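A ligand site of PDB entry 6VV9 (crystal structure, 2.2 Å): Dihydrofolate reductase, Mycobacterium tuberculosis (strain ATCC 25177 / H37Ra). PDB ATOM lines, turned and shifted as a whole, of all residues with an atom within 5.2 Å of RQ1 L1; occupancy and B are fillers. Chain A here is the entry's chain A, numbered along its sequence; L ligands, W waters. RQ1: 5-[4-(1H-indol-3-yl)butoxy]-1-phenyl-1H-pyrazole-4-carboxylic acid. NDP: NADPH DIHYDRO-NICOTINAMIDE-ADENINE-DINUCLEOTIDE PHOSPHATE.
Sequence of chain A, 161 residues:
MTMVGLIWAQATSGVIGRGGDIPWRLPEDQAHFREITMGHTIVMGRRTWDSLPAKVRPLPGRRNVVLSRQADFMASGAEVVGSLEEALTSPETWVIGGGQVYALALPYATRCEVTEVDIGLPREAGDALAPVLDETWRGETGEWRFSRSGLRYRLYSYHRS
Merely in contact with RQ1 L1: Val 56 (3.2 Å), Gln 30 (3.2 Å), Leu 59 (3.4 Å), Leu 52 (3.6 Å), Phe 33 (3.6 Å), Ile 96 (3.6 Å), Arg 25 (3.9 Å) and Pro 53 (3.97 Å).
Of the 15 residues printed, 10 come within 4 Å of RQ1 L1.
The nearest printed residue that does not touch RQ1 L1 is Thr 48 (4.01 Å).
Water W1 lies within hydrogen-bond range of N22 of RQ1 L1 (2.5 Å) and O7N of NDP L2 (3.5 Å).
O of Pro 60 is in hydrogen-bond range of NE of Arg 62 (3.0 Å).
An oxygen (O01) of RQ1 L1 lies within salt-bridge range of the guanidinium group of Arg 34 (3.7 Å).
O1A of NDP L2 is in hydrogen-bond range of OG1 of Thr 48 (2.7 Å).
NH2 of Arg 62 is in salt-bridge range of O01 of RQ1 L1 (2.9 Å).
O1A of NDP L2 sits at hydrogen-bond distance from N of Thr 48, at 3.1 Å.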
ATOM      1  N   ILE A  22     -22.083 -31.333  -4.123  1.00  0.00           N
ATOM      2  CA  ILE A  22     -21.166 -31.420  -5.254  1.00  0.00           C
ATOM      3  C   ILE A  22     -19.759 -31.652  -4.711  1.00  0.00           C
ATOM      4  O   ILE A  22     -19.335 -30.922  -3.808  1.00  0.00           O
ATOM      5  CB  ILE A  22     -21.252 -30.136  -6.106  1.00  0.00           C
ATOM      6  CG1 ILE A  22     -22.739 -29.743  -6.286  1.00  0.00           C
ATOM      7  CG2 ILE A  22     -20.491 -30.270  -7.407  1.00  0.00           C
ATOM      8  CD1 ILE A  22     -22.953 -28.474  -7.055  1.00  0.00           C
ATOM      9  N   ARG A  25     -15.521 -27.497  -5.821  1.00  0.00           N
ATOM     10  CA  ARG A  25     -15.956 -26.111  -5.848  1.00  0.00           C
ATOM     11  C   ARG A  25     -14.917 -25.314  -6.611  1.00  0.00           C
ATOM     12  O   ARG A  25     -13.744 -25.262  -6.207  1.00  0.00           O
ATOM     13  CB  ARG A  25     -16.155 -25.558  -4.434  1.00  0.00           C
ATOM     14  CG  ARG A  25     -16.941 -24.263  -4.458  1.00  0.00           C
ATOM     15  CD  ARG A  25     -17.615 -23.940  -3.117  1.00  0.00           C
ATOM     16  NE  ARG A  25     -18.605 -24.904  -2.653  1.00  0.00           N
ATOM     17  CZ  ARG A  25     -19.299 -24.734  -1.533  1.00  0.00           C
ATOM     18  NH1 ARG A  25     -19.071 -23.660  -0.812  1.00  0.00           N
ATOM     19  NH2 ARG A  25     -20.210 -25.629  -1.118  1.00  0.00           N
ATOM     20  N   ASP A  29     -16.147 -21.125 -11.899  1.00  0.00           N
ATOM     21  CA  ASP A  29     -17.401 -21.612 -12.478  1.00  0.00           C
ATOM     22  C   ASP A  29     -18.608 -20.968 -11.807  1.00  0.00           C
ATOM     23  O   ASP A  29     -19.644 -20.772 -12.460  1.00  0.00           O
ATOM     24  CB  ASP A  29     -17.461 -23.129 -12.334  1.00  0.00           C
ATOM     25  CG  ASP A  29     -18.427 -23.772 -13.309  1.00  0.00           C
ATOM     26  OD1 ASP A  29     -18.358 -23.459 -14.523  1.00  0.00           O
ATOM     27  OD2 ASP A  29     -19.260 -24.603 -12.851  1.00  0.00           O
ATOM     28  N   GLN A  30     -18.482 -20.630 -10.516  1.00  0.00           N
ATOM     29  CA  GLN A  30     -19.516 -19.850  -9.857  1.00  0.00           C
ATOM     30  C   GLN A  30     -19.711 -18.517 -10.570  1.00  0.00           C
ATOM     31  O   GLN A  30     -20.829 -18.140 -10.919  1.00  0.00           O
ATOM     32  CB  GLN A  30     -19.153 -19.621  -8.384  1.00  0.00           C
ATOM     33  CG  GLN A  30     -18.791 -20.891  -7.612  1.00  0.00           C
ATOM     34  CD  GLN A  30     -18.827 -20.691  -6.073  1.00  0.00           C
ATOM     35  OE1 GLN A  30     -18.576 -19.577  -5.560  1.00  0.00           O
ATOM     36  NE2 GLN A  30     -19.214 -21.747  -5.353  1.00  0.00           N
ATOM     37  N   PHE A  33     -21.230 -19.174 -13.751  1.00  0.00           N
ATOM     38  CA  PHE A  33     -22.638 -19.477 -13.510  1.00  0.00           C
ATOM     39  C   PHE A  33     -23.445 -18.212 -13.297  1.00  0.00           C
ATOM     40  O   PHE A  33     -24.487 -18.010 -13.945  1.00  0.00           O
ATOM     41  CB  PHE A  33     -22.762 -20.421 -12.296  1.00  0.00           C
ATOM     42  CG  PHE A  33     -24.200 -20.707 -11.875  1.00  0.00           C
ATOM     43  CD1 PHE A  33     -24.907 -21.762 -12.449  1.00  0.00           C
ATOM     44  CD2 PHE A  33     -24.824 -19.927 -10.912  1.00  0.00           C
ATOM     45  CE1 PHE A  33     -26.205 -22.022 -12.078  1.00  0.00           C
ATOM     46  CE2 PHE A  33     -26.124 -20.173 -10.525  1.00  0.00           C
ATOM     47  CZ  PHE A  33     -26.819 -21.232 -11.116  1.00  0.00           C
ATOM     48  N   ARG A  34     -22.968 -17.324 -12.404  1.00  0.00           N
ATOM     49  CA  ARG A  34     -23.640 -16.055 -12.119  1.00  0.00           C
ATOM     50  C   ARG A  34     -23.783 -15.190 -13.367  1.00  0.00           C
ATOM     51  O   ARG A  34     -24.848 -14.618 -13.611  1.00  0.00           O
ATOM     52  CB  ARG A  34     -22.866 -15.297 -11.033  1.00  0.00           C
ATOM     53  CG  ARG A  34     -23.233 -13.813 -10.907  1.00  0.00           C
ATOM     54  CD  ARG A  34     -22.915 -13.210  -9.521  1.00  0.00           C
ATOM     55  NE  ARG A  34     -23.269 -11.782  -9.447  1.00  0.00           N
ATOM     56  CZ  ARG A  34     -23.832 -11.197  -8.378  1.00  0.00           C
ATOM     57  NH1 ARG A  34     -24.111 -11.910  -7.291  1.00  0.00           N
ATOM     58  NH2 ARG A  34     -24.137  -9.896  -8.400  1.00  0.00           N
ATOM     59  N   THR A  48     -31.992 -29.562  -5.322  1.00  0.00           N
ATOM     60  CA  THR A  48     -31.007 -28.501  -5.528  1.00  0.00           C
ATOM     61  C   THR A  48     -31.299 -27.273  -4.666  1.00  0.00           C
ATOM     62  O   THR A  48     -30.370 -26.688  -4.065  1.00  0.00           O
ATOM     63  CB  THR A  48     -30.934 -28.162  -7.026  1.00  0.00           C
ATOM     64  OG1 THR A  48     -30.628 -29.349  -7.761  1.00  0.00           O
ATOM     65  CG2 THR A  48     -29.857 -27.139  -7.296  1.00  0.00           C
ATOM     66  N   SER A  51     -30.069 -27.933  -1.352  1.00  0.00           N
ATOM     67  CA  SER A  51     -28.610 -27.847  -1.301  1.00  0.00           C
ATOM     68  C   SER A  51     -28.105 -26.410  -1.163  1.00  0.00           C
ATOM     69  O   SER A  51     -26.901 -26.216  -1.000  1.00  0.00           O
ATOM     70  CB  SER A  51     -28.008 -28.512  -2.543  1.00  0.00           C
ATOM     71  OG  SER A  51     -27.815 -27.572  -3.586  1.00  0.00           O
ATOM     72  N   LEU A  52     -29.000 -25.402  -1.216  1.00  0.00           N
ATOM     73  CA  LEU A  52     -28.576 -24.008  -1.231  1.00  0.00           C
ATOM     74  C   LEU A  52     -28.654 -23.397   0.169  1.00  0.00           C
ATOM     75  O   LEU A  52     -29.718 -23.431   0.802  1.00  0.00           O
ATOM     76  CB  LEU A  52     -29.428 -23.205  -2.187  1.00  0.00           C
ATOM     77  CG  LEU A  52     -28.958 -23.120  -3.648  1.00  0.00           C
ATOM     78  CD1 LEU A  52     -30.002 -22.397  -4.478  1.00  0.00           C
ATOM     79  CD2 LEU A  52     -27.604 -22.436  -3.767  1.00  0.00           C
ATOM     80  N   PRO A  53     -27.555 -22.831   0.674  1.00  0.00           N
ATOM     81  CA  PRO A  53     -27.585 -22.203   1.998  1.00  0.00           C
ATOM     82  C   PRO A  53     -28.608 -21.086   2.073  1.00  0.00           C
ATOM     83  O   PRO A  53     -28.940 -20.444   1.069  1.00  0.00           O
ATOM     84  CB  PRO A  53     -26.160 -21.666   2.168  1.00  0.00           C
ATOM     85  CG  PRO A  53     -25.316 -22.553   1.249  1.00  0.00           C
ATOM     86  CD  PRO A  53     -26.200 -22.888   0.083  1.00  0.00           C
ATOM     87  N   VAL A  56     -27.775 -17.647   0.881  1.00  0.00           N
ATOM     88  CA  VAL A  56     -27.691 -17.472  -0.573  1.00  0.00           C
ATOM     89  C   VAL A  56     -29.066 -17.444  -1.251  1.00  0.00           C
ATOM     90  O   VAL A  56     -29.199 -16.850  -2.327  1.00  0.00           O
ATOM     91  CB  VAL A  56     -26.789 -18.573  -1.143  1.00  0.00           C
ATOM     92  CG1 VAL A  56     -26.703 -18.485  -2.642  1.00  0.00           C
ATOM     93  CG2 VAL A  56     -25.403 -18.461  -0.548  1.00  0.00           C
ATOM     94  N   LEU A  59     -31.199 -16.929  -5.307  1.00  0.00           N
ATOM     95  CA  LEU A  59     -30.057 -16.383  -6.038  1.00  0.00           C
ATOM     96  C   LEU A  59     -30.419 -14.978  -6.518  1.00  0.00           C
ATOM     97  O   LEU A  59     -31.402 -14.822  -7.270  1.00  0.00           O
ATOM     98  CB  LEU A  59     -29.659 -17.292  -7.202  1.00  0.00           C
ATOM     99  CG  LEU A  59     -28.987 -18.595  -6.777  1.00  0.00           C
ATOM    100  CD1 LEU A  59     -28.781 -19.528  -7.960  1.00  0.00           C
ATOM    101  CD2 LEU A  59     -27.663 -18.300  -6.069  1.00  0.00           C
ATOM    102  N   PRO A  60     -29.698 -13.943  -6.100  1.00  0.00           N
ATOM    103  CA  PRO A  60     -30.210 -12.584  -6.276  1.00  0.00           C
ATOM    104  C   PRO A  60     -30.188 -12.169  -7.745  1.00  0.00           C
ATOM    105  O   PRO A  60     -29.345 -12.597  -8.522  1.00  0.00           O
ATOM    106  CB  PRO A  60     -29.244 -11.740  -5.426  1.00  0.00           C
ATOM    107  CG  PRO A  60     -27.968 -12.534  -5.391  1.00  0.00           C
ATOM    108  CD  PRO A  60     -28.364 -13.981  -5.467  1.00  0.00           C
ATOM    109  N   ARG A  62     -32.438 -12.844 -10.062  1.00  0.00           N
ATOM    110  CA  ARG A  62     -32.994 -13.874 -10.917  1.00  0.00           C
ATOM    111  C   ARG A  62     -34.346 -14.276 -10.363  1.00  0.00           C
ATOM    112  O   ARG A  62     -34.674 -13.997  -9.201  1.00  0.00           O
ATOM    113  CB  ARG A  62     -32.076 -15.096 -10.983  1.00  0.00           C
ATOM    114  CG  ARG A  62     -30.807 -14.863 -11.786  1.00  0.00           C
ATOM    115  CD  ARG A  62     -29.645 -15.692 -11.285  1.00  0.00           C
ATOM    116  NE  ARG A  62     -29.054 -15.129 -10.083  1.00  0.00           N
ATOM    117  CZ  ARG A  62     -27.848 -15.461  -9.627  1.00  0.00           C
ATOM    118  NH1 ARG A  62     -27.111 -16.348 -10.301  1.00  0.00           N
ATOM    119  NH2 ARG A  62     -27.374 -14.919  -8.496  1.00  0.00           N
ATOM    120  N   ILE A  96     -30.928 -25.246 -13.788  1.00  0.00           N
ATOM    121  CA  ILE A  96     -29.686 -25.254 -13.033  1.00  0.00           C
ATOM    122  C   ILE A  96     -29.505 -26.538 -12.228  1.00  0.00           C
ATOM    123  O   ILE A  96     -28.556 -26.636 -11.431  1.00  0.00           O
ATOM    124  CB  ILE A  96     -29.545 -24.009 -12.139  1.00  0.00           C
ATOM    125  CG1 ILE A  96     -30.395 -24.072 -10.892  1.00  0.00           C
ATOM    126  CG2 ILE A  96     -29.843 -22.745 -12.895  1.00  0.00           C
ATOM    127  CD1 ILE A  96     -29.891 -23.103  -9.867  1.00  0.00           C
HETATM  128  C10 RQ1 L   1     -23.802 -22.416  -3.045  1.00  0.00           C
HETATM  129  C13 RQ1 L   1     -22.008 -20.390  -3.596  1.00  0.00           C
HETATM  130  C17 RQ1 L   1     -22.338 -21.265  -7.807  1.00  0.00           C
HETATM  131  C20 RQ1 L   1     -22.792 -24.063  -8.985  1.00  0.00           C
HETATM  132  C21 RQ1 L   1     -22.874 -24.420 -10.317  1.00  0.00           C
HETATM  133  C24 RQ1 L   1     -26.260 -24.812  -9.267  1.00  0.00           C
HETATM  134  C26 RQ1 L   1     -26.021 -24.194  -6.984  1.00  0.00           C
HETATM  135  C28 RQ1 L   1     -24.087 -24.175  -8.438  1.00  0.00           C
HETATM  136  C02 RQ1 L   1     -24.754 -16.758  -7.233  1.00  0.00           C
HETATM  137  C04 RQ1 L   1     -24.342 -17.538  -5.974  1.00  0.00           C
HETATM  138  C05 RQ1 L   1     -24.252 -17.028  -4.709  1.00  0.00           C
HETATM  139  C08 RQ1 L   1     -23.328 -20.266  -4.011  1.00  0.00           C
HETATM  140  C09 RQ1 L   1     -24.225 -21.282  -3.715  1.00  0.00           C
HETATM  141  C11 RQ1 L   1     -22.488 -22.534  -2.642  1.00  0.00           C
HETATM  142  C12 RQ1 L   1     -21.598 -21.520  -2.925  1.00  0.00           C
HETATM  143  C14 RQ1 L   1     -23.999 -18.887  -5.917  1.00  0.00           C
HETATM  144  C16 RQ1 L   1     -23.620 -21.000  -7.036  1.00  0.00           C
HETATM  145  C18 RQ1 L   1     -21.725 -22.551  -7.248  1.00  0.00           C
HETATM  146  C19 RQ1 L   1     -21.504 -23.639  -8.290  1.00  0.00           C
HETATM  147  C23 RQ1 L   1     -24.893 -24.598  -9.471  1.00  0.00           C
HETATM  148  C25 RQ1 L   1     -26.832 -24.612  -8.029  1.00  0.00           C
HETATM  149  C27 RQ1 L   1     -24.669 -23.984  -7.182  1.00  0.00           C
HETATM  150  N06 RQ1 L   1     -23.862 -18.008  -3.919  1.00  0.00           N
HETATM  151  N07 RQ1 L   1     -23.707 -19.157  -4.630  1.00  0.00           N
HETATM  152  N22 RQ1 L   1     -24.136 -24.730 -10.570  1.00  0.00           N
HETATM  153  O01 RQ1 L   1     -24.868 -15.512  -7.155  1.00  0.00           O
HETATM  154  O03 RQ1 L   1     -24.987 -17.337  -8.321  1.00  0.00           O
HETATM  155  O15 RQ1 L   1     -24.003 -19.660  -7.087  1.00  0.00           O
HETATM  156  PA  NDP L   2     -33.281 -32.580  -8.120  1.00  0.00           P
HETATM  157  O1A NDP L   2     -32.453 -31.382  -7.736  1.00  0.00           O
HETATM  158  O2A NDP L   2     -33.414 -32.755  -9.622  1.00  0.00           O
HETATM  159  O5B NDP L   2     -34.763 -32.430  -7.487  1.00  0.00           O
HETATM  160  C5B NDP L   2     -35.603 -33.504  -7.648  1.00  0.00           C
HETATM  161  C4B NDP L   2     -36.856 -32.965  -6.980  1.00  0.00           C
HETATM  162  O4B NDP L   2     -37.500 -32.140  -7.797  1.00  0.00           O
HETATM  163  C3B NDP L   2     -37.819 -34.105  -6.618  1.00  0.00           C
HETATM  164  O3B NDP L   2     -37.588 -34.505  -5.322  1.00  0.00           O
HETATM  165  C2B NDP L   2     -39.181 -33.391  -6.789  1.00  0.00           C
HETATM  166  O2B NDP L   2     -39.409 -32.558  -5.592  1.00  0.00           O
HETATM  167  C1B NDP L   2     -39.036 -32.563  -7.794  1.00  0.00           C
HETATM  168  N9A NDP L   2     -39.243 -33.246  -9.025  1.00  0.00           N
HETATM  169  C8A NDP L   2     -38.585 -34.146  -9.761  1.00  0.00           C
HETATM  170  N7A NDP L   2     -39.310 -34.369 -10.858  1.00  0.00           N
HETATM  171  C5A NDP L   2     -40.414 -33.621 -10.803  1.00  0.00           C
HETATM  172  C6A NDP L   2     -41.470 -33.483 -11.657  1.00  0.00           C
HETATM  173  N6A NDP L   2     -41.799 -34.079 -12.922  1.00  0.00           N
HETATM  174  N1A NDP L   2     -42.465 -32.655 -11.358  1.00  0.00           N
HETATM  175  C2A NDP L   2     -42.460 -31.926 -10.210  1.00  0.00           C
HETATM  176  N3A NDP L   2     -41.409 -32.080  -9.379  1.00  0.00           N
HETATM  177  C4A NDP L   2     -40.386 -32.916  -9.661  1.00  0.00           C
HETATM  178  O3  NDP L   2     -32.677 -33.947  -7.484  1.00  0.00           O
HETATM  179  PN  NDP L   2     -31.195 -34.501  -7.902  1.00  0.00           P
HETATM  180  O1N NDP L   2     -31.002 -35.858  -7.304  1.00  0.00           O
HETATM  181  O2N NDP L   2     -31.094 -34.657  -9.408  1.00  0.00           O
HETATM  182  O5D NDP L   2     -30.205 -33.449  -7.125  1.00  0.00           O
HETATM  183  C5D NDP L   2     -29.232 -32.680  -7.730  1.00  0.00           C
HETATM  184  C4D NDP L   2     -27.885 -33.189  -7.199  1.00  0.00           C
HETATM  185  O4D NDP L   2     -26.970 -32.779  -8.056  1.00  0.00           O
HETATM  186  C3D NDP L   2     -27.477 -32.580  -5.854  1.00  0.00           C
HETATM  187  O3D NDP L   2     -26.431 -33.277  -5.343  1.00  0.00           O
HETATM  188  C2D NDP L   2     -26.872 -31.227  -6.243  1.00  0.00           C
HETATM  189  O2D NDP L   2     -25.858 -30.922  -5.217  1.00  0.00           O
HETATM  190  C1D NDP L   2     -26.273 -31.514  -7.399  1.00  0.00           C
HETATM  191  N1N NDP L   2     -26.272 -30.429  -8.359  1.00  0.00           N
HETATM  192  C2N NDP L   2     -25.123 -30.297  -9.187  1.00  0.00           C
HETATM  193  C3N NDP L   2     -25.031 -29.294 -10.286  1.00  0.00           C
HETATM  194  C7N NDP L   2     -23.711 -29.091 -11.009  1.00  0.00           C
HETATM  195  O7N NDP L   2     -23.606 -28.160 -11.744  1.00  0.00           O
HETATM  196  N7N NDP L   2     -22.615 -30.027 -10.823  1.00  0.00           N
HETATM  197  C4N NDP L   2     -26.148 -28.231 -10.451  1.00  0.00           C
HETATM  198  C5N NDP L   2     -27.468 -28.659  -9.718  1.00  0.00           C
HETATM  199  C6N NDP L   2     -27.407 -29.552  -8.485  1.00  0.00           C
HETATM  200  P2B NDP L   2     -40.254 -33.244  -4.379  1.00  0.00           P
HETATM  201  O1X NDP L   2     -40.186 -32.362  -3.143  1.00  0.00           O
HETATM  202  O2X NDP L   2     -39.584 -34.550  -4.092  1.00  0.00           O
HETATM  203  O3X NDP L   2     -41.689 -33.483  -4.820  1.00  0.00           O
HETATM  204  O   HOH W   1     -23.703 -24.943 -13.017  1.00  0.00           O
